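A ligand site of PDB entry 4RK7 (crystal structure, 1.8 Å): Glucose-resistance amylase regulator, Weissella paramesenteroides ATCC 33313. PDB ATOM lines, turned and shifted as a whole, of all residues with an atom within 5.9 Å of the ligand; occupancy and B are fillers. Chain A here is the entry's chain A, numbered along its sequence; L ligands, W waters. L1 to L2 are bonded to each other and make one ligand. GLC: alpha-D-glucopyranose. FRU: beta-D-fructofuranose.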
ATOM      1  N   THR A  22      -9.285  27.853   6.251  1.00  0.00           N
ATOM      2  CA  THR A  22     -10.392  28.624   5.682  1.00  0.00           C
ATOM      3  C   THR A  22     -11.595  28.480   6.648  1.00  0.00           C
ATOM      4  O   THR A  22     -11.573  27.641   7.564  1.00  0.00           O
ATOM      5  CB  THR A  22     -10.775  28.094   4.261  1.00  0.00           C
ATOM      6  OG1 THR A  22      -9.623  28.079   3.384  1.00  0.00           O
ATOM      7  CG2 THR A  22     -11.864  28.949   3.627  1.00  0.00           C
ATOM      8  N   PHE A  24     -14.109  26.915   6.020  1.00  0.00           N
ATOM      9  CA  PHE A  24     -14.789  25.653   5.750  1.00  0.00           C
ATOM     10  C   PHE A  24     -15.018  24.858   7.043  1.00  0.00           C
ATOM     11  O   PHE A  24     -16.060  24.226   7.201  1.00  0.00           O
ATOM     12  CB  PHE A  24     -14.088  24.832   4.632  1.00  0.00           C
ATOM     13  CG  PHE A  24     -12.994  23.933   5.111  1.00  0.00           C
ATOM     14  CD1 PHE A  24     -11.685  24.391   5.189  1.00  0.00           C
ATOM     15  CD2 PHE A  24     -13.260  22.619   5.438  1.00  0.00           C
ATOM     16  CE1 PHE A  24     -10.676  23.545   5.637  1.00  0.00           C
ATOM     17  CE2 PHE A  24     -12.256  21.774   5.862  1.00  0.00           C
ATOM     18  CZ  PHE A  24     -10.961  22.237   5.973  1.00  0.00           C
ATOM     19  N   LEU A  73      -9.839  16.920   9.943  1.00  0.00           N
ATOM     20  CA  LEU A  73     -10.085  17.893   8.919  1.00  0.00           C
ATOM     21  C   LEU A  73      -8.778  18.411   8.297  1.00  0.00           C
ATOM     22  O   LEU A  73      -8.831  19.271   7.431  1.00  0.00           O
ATOM     23  CB  LEU A  73     -10.866  19.075   9.510  1.00  0.00           C
ATOM     24  CG  LEU A  73     -12.384  18.958   9.627  1.00  0.00           C
ATOM     25  CD1 LEU A  73     -12.790  17.786  10.510  1.00  0.00           C
ATOM     26  CD2 LEU A  73     -12.955  20.266  10.162  1.00  0.00           C
ATOM     27  N   SER A  74      -7.630  17.877   8.727  1.00  0.00           N
ATOM     28  CA  SER A  74      -6.297  18.402   8.342  1.00  0.00           C
ATOM     29  C   SER A  74      -5.473  17.329   7.636  1.00  0.00           C
ATOM     30  O   SER A  74      -5.487  16.175   8.047  1.00  0.00           O
ATOM     31  CB  SER A  74      -5.533  18.846   9.601  1.00  0.00           C
ATOM     32  OG  SER A  74      -4.159  19.130   9.337  1.00  0.00           O
ATOM     33  N   LEU A  75      -4.737  17.706   6.590  1.00  0.00           N
ATOM     34  CA  LEU A  75      -3.865  16.732   5.917  1.00  0.00           C
ATOM     35  C   LEU A  75      -2.526  16.542   6.635  1.00  0.00           C
ATOM     36  O   LEU A  75      -1.774  15.635   6.306  1.00  0.00           O
ATOM     37  CB  LEU A  75      -3.662  17.072   4.433  1.00  0.00           C
ATOM     38  CG  LEU A  75      -4.642  16.366   3.474  1.00  0.00           C
ATOM     39  CD1 LEU A  75      -4.439  16.864   2.056  1.00  0.00           C
ATOM     40  CD2 LEU A  75      -4.480  14.854   3.524  1.00  0.00           C
ATOM     41  N   LEU A  95     -12.505  14.133   6.862  1.00  0.00           N
ATOM     42  CA  LEU A  95     -13.479  14.958   6.165  1.00  0.00           C
ATOM     43  C   LEU A  95     -12.787  15.917   5.205  1.00  0.00           C
ATOM     44  O   LEU A  95     -11.877  16.631   5.617  1.00  0.00           O
ATOM     45  CB  LEU A  95     -14.277  15.773   7.178  1.00  0.00           C
ATOM     46  CG  LEU A  95     -15.333  14.982   7.983  1.00  0.00           C
ATOM     47  CD1 LEU A  95     -14.723  13.983   8.924  1.00  0.00           C
ATOM     48  CD2 LEU A  95     -16.197  15.953   8.784  1.00  0.00           C
ATOM     49  N   THR A  96     -13.280  15.943   3.968  1.00  0.00           N
ATOM     50  CA  THR A  96     -12.805  16.785   2.848  1.00  0.00           C
ATOM     51  C   THR A  96     -11.440  16.369   2.291  1.00  0.00           C
ATOM     52  O   THR A  96     -10.900  17.018   1.419  1.00  0.00           O
ATOM     53  CB  THR A  96     -12.795  18.300   3.162  1.00  0.00           C
ATOM     54  OG1 THR A  96     -11.642  18.644   3.928  1.00  0.00           O
ATOM     55  CG2 THR A  96     -14.067  18.708   3.865  1.00  0.00           C
ATOM     56  N   ALA A  97     -10.929  15.246   2.767  1.00  0.00           N
ATOM     57  CA  ALA A  97      -9.612  14.789   2.356  1.00  0.00           C
ATOM     58  C   ALA A  97      -9.508  13.300   2.648  1.00  0.00           C
ATOM     59  O   ALA A  97     -10.139  12.803   3.573  1.00  0.00           O
ATOM     60  CB  ALA A  97      -8.540  15.555   3.109  1.00  0.00           C
ATOM     61  N   GLU A 110     -13.090  15.481  -5.605  1.00  0.00           N
ATOM     62  CA  GLU A 110     -12.159  16.511  -6.120  1.00  0.00           C
ATOM     63  C   GLU A 110     -12.046  16.579  -7.628  1.00  0.00           C
ATOM     64  O   GLU A 110     -12.056  17.679  -8.197  1.00  0.00           O
ATOM     65  CB  GLU A 110     -10.782  16.340  -5.485  1.00  0.00           C
ATOM     66  CG  GLU A 110     -10.743  16.754  -4.027  1.00  0.00           C
ATOM     67  CD  GLU A 110     -10.509  18.260  -3.845  1.00  0.00           C
ATOM     68  OE1 GLU A 110     -10.254  18.989  -4.830  1.00  0.00           O
ATOM     69  OE2 GLU A 110     -10.535  18.684  -2.695  1.00  0.00           O
ATOM     70  N   MET A 113     -15.291  18.058  -9.099  1.00  0.00           N
ATOM     71  CA  MET A 113     -15.321  19.512  -8.881  1.00  0.00           C
ATOM     72  C   MET A 113     -14.487  20.207  -9.906  1.00  0.00           C
ATOM     73  O   MET A 113     -14.974  21.105 -10.614  1.00  0.00           O
ATOM     74  CB  MET A 113     -14.802  19.941  -7.521  1.00  0.00           C
ATOM     75  CG  MET A 113     -15.730  19.597  -6.369  1.00  0.00           C
ATOM     76  SD  MET A 113     -15.267  20.615  -4.755  1.00  0.00           S
ATOM     77  CE  MET A 113     -13.690  19.582  -4.209  1.00  0.00           C
ATOM     78  N   ASP A 134      -3.408  26.826  -3.834  1.00  0.00           N
ATOM     79  CA  ASP A 134      -2.551  25.729  -3.407  1.00  0.00           C
ATOM     80  C   ASP A 134      -2.214  24.845  -4.608  1.00  0.00           C
ATOM     81  O   ASP A 134      -2.977  23.963  -4.954  1.00  0.00           O
ATOM     82  CB  ASP A 134      -3.278  24.926  -2.310  1.00  0.00           C
ATOM     83  CG  ASP A 134      -2.412  23.851  -1.694  1.00  0.00           C
ATOM     84  OD1 ASP A 134      -1.248  23.686  -2.094  1.00  0.00           O
ATOM     85  OD2 ASP A 134      -2.912  23.164  -0.796  1.00  0.00           O
ATOM     86  N   ILE A 141       2.492  15.320   0.726  1.00  0.00           N
ATOM     87  CA  ILE A 141       1.064  15.621   0.474  1.00  0.00           C
ATOM     88  C   ILE A 141       0.776  15.645  -1.003  1.00  0.00           C
ATOM     89  O   ILE A 141       1.402  16.403  -1.748  1.00  0.00           O
ATOM     90  CB  ILE A 141       0.649  16.997   1.074  1.00  0.00           C
ATOM     91  CG1 ILE A 141       1.020  17.100   2.576  1.00  0.00           C
ATOM     92  CG2 ILE A 141      -0.828  17.274   0.866  1.00  0.00           C
ATOM     93  CD1 ILE A 141       0.314  16.116   3.479  1.00  0.00           C
ATOM     94  N   SER A 142      -0.210  14.860  -1.420  1.00  0.00           N
ATOM     95  CA  SER A 142      -0.661  14.841  -2.808  1.00  0.00           C
ATOM     96  C   SER A 142      -1.066  16.249  -3.225  1.00  0.00           C
ATOM     97  O   SER A 142      -1.716  16.961  -2.459  1.00  0.00           O
ATOM     98  CB  SER A 142      -1.882  13.923  -2.932  1.00  0.00           C
ATOM     99  OG  SER A 142      -1.628  12.638  -2.409  1.00  0.00           O
ATOM    100  N   THR A 144      -3.413  17.512  -4.979  1.00  0.00           N
ATOM    101  CA  THR A 144      -4.692  17.058  -5.522  1.00  0.00           C
ATOM    102  C   THR A 144      -5.231  17.963  -6.608  1.00  0.00           C
ATOM    103  O   THR A 144      -5.516  17.519  -7.713  1.00  0.00           O
ATOM    104  CB  THR A 144      -5.703  16.955  -4.362  1.00  0.00           C
ATOM    105  OG1 THR A 144      -5.192  16.062  -3.366  1.00  0.00           O
ATOM    106  CG2 THR A 144      -7.077  16.475  -4.869  1.00  0.00           C
ATOM    107  N   ARG A 145      -5.343  19.255  -6.312  1.00  0.00           N
ATOM    108  CA  ARG A 145      -5.934  20.179  -7.279  1.00  0.00           C
ATOM    109  C   ARG A 145      -5.108  20.476  -8.516  1.00  0.00           C
ATOM    110  O   ARG A 145      -5.628  20.537  -9.627  1.00  0.00           O
ATOM    111  CB  ARG A 145      -6.405  21.447  -6.561  1.00  0.00           C
ATOM    112  CG  ARG A 145      -7.542  21.070  -5.644  1.00  0.00           C
ATOM    113  CD  ARG A 145      -8.317  22.244  -5.021  1.00  0.00           C
ATOM    114  NE  ARG A 145      -9.415  21.648  -4.243  1.00  0.00           N
ATOM    115  CZ  ARG A 145     -10.112  22.242  -3.290  1.00  0.00           C
ATOM    116  NH1 ARG A 145      -9.909  23.519  -2.950  1.00  0.00           N
ATOM    117  NH2 ARG A 145     -11.029  21.528  -2.646  1.00  0.00           N
ATOM    118  N   HIS A 170      -3.989  28.807   0.138  1.00  0.00           N
ATOM    119  CA  HIS A 170      -5.345  29.254  -0.203  1.00  0.00           C
ATOM    120  C   HIS A 170      -5.629  30.702   0.233  1.00  0.00           C
ATOM    121  O   HIS A 170      -6.794  31.061   0.412  1.00  0.00           O
ATOM    122  CB  HIS A 170      -6.373  28.340   0.494  1.00  0.00           C
ATOM    123  CG  HIS A 170      -6.355  26.913   0.037  1.00  0.00           C
ATOM    124  ND1 HIS A 170      -6.673  26.539  -1.253  1.00  0.00           N
ATOM    125  CD2 HIS A 170      -6.131  25.765   0.720  1.00  0.00           C
ATOM    126  CE1 HIS A 170      -6.596  25.220  -1.355  1.00  0.00           C
ATOM    127  NE2 HIS A 170      -6.279  24.726  -0.170  1.00  0.00           N
ATOM    128  N   THR A 196      -8.312  28.169  -5.876  1.00  0.00           N
ATOM    129  CA  THR A 196      -8.511  26.961  -5.065  1.00  0.00           C
ATOM    130  C   THR A 196      -9.304  27.180  -3.772  1.00  0.00           C
ATOM    131  O   THR A 196      -9.688  26.222  -3.110  1.00  0.00           O
ATOM    132  CB  THR A 196      -7.174  26.265  -4.703  1.00  0.00           C
ATOM    133  OG1 THR A 196      -6.379  27.116  -3.876  1.00  0.00           O
ATOM    134  CG2 THR A 196      -6.425  25.911  -5.940  1.00  0.00           C
ATOM    135  N   ALA A 197      -9.532  28.445  -3.409  1.00  0.00           N
ATOM    136  CA  ALA A 197     -10.432  28.808  -2.291  1.00  0.00           C
ATOM    137  C   ALA A 197     -11.042  30.179  -2.579  1.00  0.00           C
ATOM    138  O   ALA A 197     -10.523  30.937  -3.409  1.00  0.00           O
ATOM    139  CB  ALA A 197      -9.668  28.827  -0.992  1.00  0.00           C
ATOM    140  N   ILE A 224     -13.401  27.648  -5.666  1.00  0.00           N
ATOM    141  CA  ILE A 224     -13.852  26.427  -4.999  1.00  0.00           C
ATOM    142  C   ILE A 224     -14.167  26.762  -3.549  1.00  0.00           C
ATOM    143  O   ILE A 224     -13.336  27.342  -2.863  1.00  0.00           O
ATOM    144  CB  ILE A 224     -12.806  25.305  -5.092  1.00  0.00           C
ATOM    145  CG1 ILE A 224     -12.623  24.898  -6.564  1.00  0.00           C
ATOM    146  CG2 ILE A 224     -13.248  24.124  -4.236  1.00  0.00           C
ATOM    147  CD1 ILE A 224     -11.353  24.103  -6.811  1.00  0.00           C
ATOM    148  N   ASP A 225     -15.408  26.428  -3.142  1.00  0.00           N
ATOM    149  CA  ASP A 225     -15.916  26.331  -1.763  1.00  0.00           C
ATOM    150  C   ASP A 225     -17.327  26.952  -1.684  1.00  0.00           C
ATOM    151  O   ASP A 225     -18.234  26.358  -1.114  1.00  0.00           O
ATOM    152  CB  ASP A 225     -15.072  26.960  -0.656  1.00  0.00           C
ATOM    153  CG  ASP A 225     -13.855  26.143  -0.292  1.00  0.00           C
ATOM    154  OD1 ASP A 225     -13.708  24.988  -0.772  1.00  0.00           O
ATOM    155  OD2 ASP A 225     -13.019  26.684   0.452  1.00  0.00           O
ATOM    156  N   GLN A 242     -19.458  23.657  -2.094  1.00  0.00           N
ATOM    157  CA  GLN A 242     -19.401  22.375  -1.357  1.00  0.00           C
ATOM    158  C   GLN A 242     -20.463  22.396  -0.281  1.00  0.00           C
ATOM    159  O   GLN A 242     -20.769  23.427   0.285  1.00  0.00           O
ATOM    160  CB  GLN A 242     -18.038  22.216  -0.697  1.00  0.00           C
ATOM    161  CG  GLN A 242     -16.886  22.127  -1.689  1.00  0.00           C
ATOM    162  CD  GLN A 242     -15.661  21.463  -1.093  1.00  0.00           C
ATOM    163  OE1 GLN A 242     -15.714  20.318  -0.694  1.00  0.00           O
ATOM    164  NE2 GLN A 242     -14.553  22.202  -0.990  1.00  0.00           N
ATOM    165  N   PHE A 244     -20.575  21.664   3.019  1.00  0.00           N
ATOM    166  CA  PHE A 244     -19.774  21.324   4.195  1.00  0.00           C
ATOM    167  C   PHE A 244     -20.639  20.791   5.336  1.00  0.00           C
ATOM    168  O   PHE A 244     -20.247  19.843   6.020  1.00  0.00           O
ATOM    169  CB  PHE A 244     -18.924  22.500   4.676  1.00  0.00           C
ATOM    170  CG  PHE A 244     -17.827  22.888   3.710  1.00  0.00           C
ATOM    171  CD1 PHE A 244     -16.857  21.965   3.351  1.00  0.00           C
ATOM    172  CD2 PHE A 244     -17.790  24.155   3.126  1.00  0.00           C
ATOM    173  CE1 PHE A 244     -15.876  22.298   2.429  1.00  0.00           C
ATOM    174  CE2 PHE A 244     -16.793  24.498   2.210  1.00  0.00           C
ATOM    175  CZ  PHE A 244     -15.842  23.559   1.866  1.00  0.00           C
HETATM  176  C1  GLC L   1      -9.130  22.228   2.380  1.00  0.00           C
HETATM  177  C2  GLC L   1     -10.414  21.446   2.184  1.00  0.00           C
HETATM  178  C3  GLC L   1     -11.006  21.752   0.818  1.00  0.00           C
HETATM  179  C4  GLC L   1     -11.171  23.264   0.665  1.00  0.00           C
HETATM  180  C5  GLC L   1      -9.840  23.975   0.857  1.00  0.00           C
HETATM  181  C6  GLC L   1      -9.946  25.515   0.767  1.00  0.00           C
HETATM  182  O2  GLC L   1     -10.126  20.040   2.284  1.00  0.00           O
HETATM  183  O3  GLC L   1     -12.263  21.060   0.627  1.00  0.00           O
HETATM  184  O4  GLC L   1     -11.661  23.549  -0.634  1.00  0.00           O
HETATM  185  O5  GLC L   1      -9.312  23.633   2.113  1.00  0.00           O
HETATM  186  O6  GLC L   1     -10.852  25.997   1.748  1.00  0.00           O
HETATM  187  C1  FRU L   2      -6.338  22.319   2.895  1.00  0.00           C
HETATM  188  C2  FRU L   2      -6.843  21.522   1.685  1.00  0.00           C
HETATM  189  C3  FRU L   2      -6.617  20.013   1.724  1.00  0.00           C
HETATM  190  C4  FRU L   2      -6.745  19.651   0.248  1.00  0.00           C
HETATM  191  C5  FRU L   2      -6.139  20.867  -0.468  1.00  0.00           C
HETATM  192  C6  FRU L   2      -6.878  21.273  -1.733  1.00  0.00           C
HETATM  193  O1  FRU L   2      -4.941  22.108   3.030  1.00  0.00           O
HETATM  194  O2  FRU L   2      -8.229  21.725   1.382  1.00  0.00           O
HETATM  195  O3  FRU L   2      -7.583  19.382   2.578  1.00  0.00           O
HETATM  196  O4  FRU L   2      -6.096  18.442  -0.155  1.00  0.00           O
HETATM  197  O5  FRU L   2      -6.142  21.920   0.517  1.00  0.00           O
HETATM  198  O6  FRU L   2      -6.184  22.320  -2.422  1.00  0.00           O
HETATM  199  O   HOH W   1      -3.490  24.110   1.785  1.00  0.00           O
HETATM  200  O   HOH W   2      -9.125  17.048  -0.747  1.00  0.00           O
HETATM  201  O   HOH W   3      -4.556  20.440  -3.622  1.00  0.00           O
HETATM  202  O   HOH W   4     -12.092  18.611  -0.398  1.00  0.00           O
HETATM  203  O   HOH W   5      -3.348  19.031  -1.615  1.00  0.00           O
HETATM  204  O   HOH W   6      -8.222  25.521   4.393  1.00  0.00           O
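The side-chain carboxylate (OD1) of Asp 225 lies within hydrogen-bond range of an oxygen (O4) of GLC L1 (2.5 Å).
The backbone carbonyl oxygen of Thr 96 sits at hydrogen-bond distance from an oxygen (O2) of GLC L1, at 3.2 Å.
The side-chain hydroxyl (OG1) of Thr 96 is in hydrogen-bond range of an oxygen (O2) of GLC L1 (2.6 Å).
NE2 of His 170 sits at hydrogen-bond distance from O5 of FRU L2, at 2.9 Å.
The guanidinium group (NH1) of Arg 145 lies within hydrogen-bond range of an oxygen (O4) of GLC L1 (2.9 Å).
The side-chain hydroxyl of Thr 22 lies within hydrogen-bond range of an oxygen (O6) of GLC L1.
NE2 of Gln 242 is in hydrogen-bond range of O3 of GLC L1.
OD1 of Asp 225 lies within hydrogen-bond range of NE2 of Gln 242 (2.9 Å).
ND1 of His 170 sits at hydrogen-bond distance from OG1 of Thr 196 (2.7 Å).
The guanidinium group of Arg 145 lies within hydrogen-bond range of the backbone carbonyl oxygen of Thr 196 (2.7 Å).
The guanidinium group (NE) of Arg 145 is in salt-bridge range of the side-chain carboxylate (OE1) of Glu 110 (2.8 Å).
The backbone NH (N) of Asp 134 sits at hydrogen-bond distance from the side-chain hydroxyl (OG1) of Thr 196 (3.0 Å).
Residues that only touch the ligand: Phe 24 (3.8 Å), Leu 75 (3.2 Å), Ala 97 (3.98 Å), Asp 134 (3.7 Å), Thr 196 (3.9 Å), Ala 197 (3.8 Å) and Ile 224 (3.98 Å).
Hydrophobic or aromatic side chains that line the ligand: Phe 24, Leu 75, Ala 97, His 170, Ala 197 and Ile 224.
13 residues have an atom within 4 Å of the ligand: Thr 22, Phe 24, Leu 75, Thr 96, Ala 97, Asp 134, Arg 145, His 170, Thr 196, Ala 197, Ile 224, Asp 225 and Gln 242.
The nearest printed residue that does not touch the ligand is Thr 144 (4.1 Å).
Water W4 lies within hydrogen-bond range of an oxygen (O3) of GLC L1 (2.7 Å), the backbone carbonyl oxygen of Thr 96 (2.7 Å) and the side-chain carboxylate of Glu 110 (2.8 Å).
Water W3 lies within hydrogen-bond range of O6 of FRU L2, N of Arg 145 and N of Thr 144.
Water W1 lies within hydrogen-bond range of O1 of FRU L2 (2.8 Å), OD2 of Asp 134 (2.8 Å) and NE2 of His 170 (3.5 Å).
Water W6 lies within hydrogen-bond range of the side-chain hydroxyl of Thr 22 and an oxygen (O5) of GLC L1.
Water W5 bridges the backbone carbonyl oxygen (O) of Ser 142 and an oxygen (O4) of FRU L2.
Water W2 lies within hydrogen-bond range of the backbone carbonyl oxygen of Thr 96, the side-chain carboxylate of Glu 110 and an oxygen (O4) of FRU L2.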
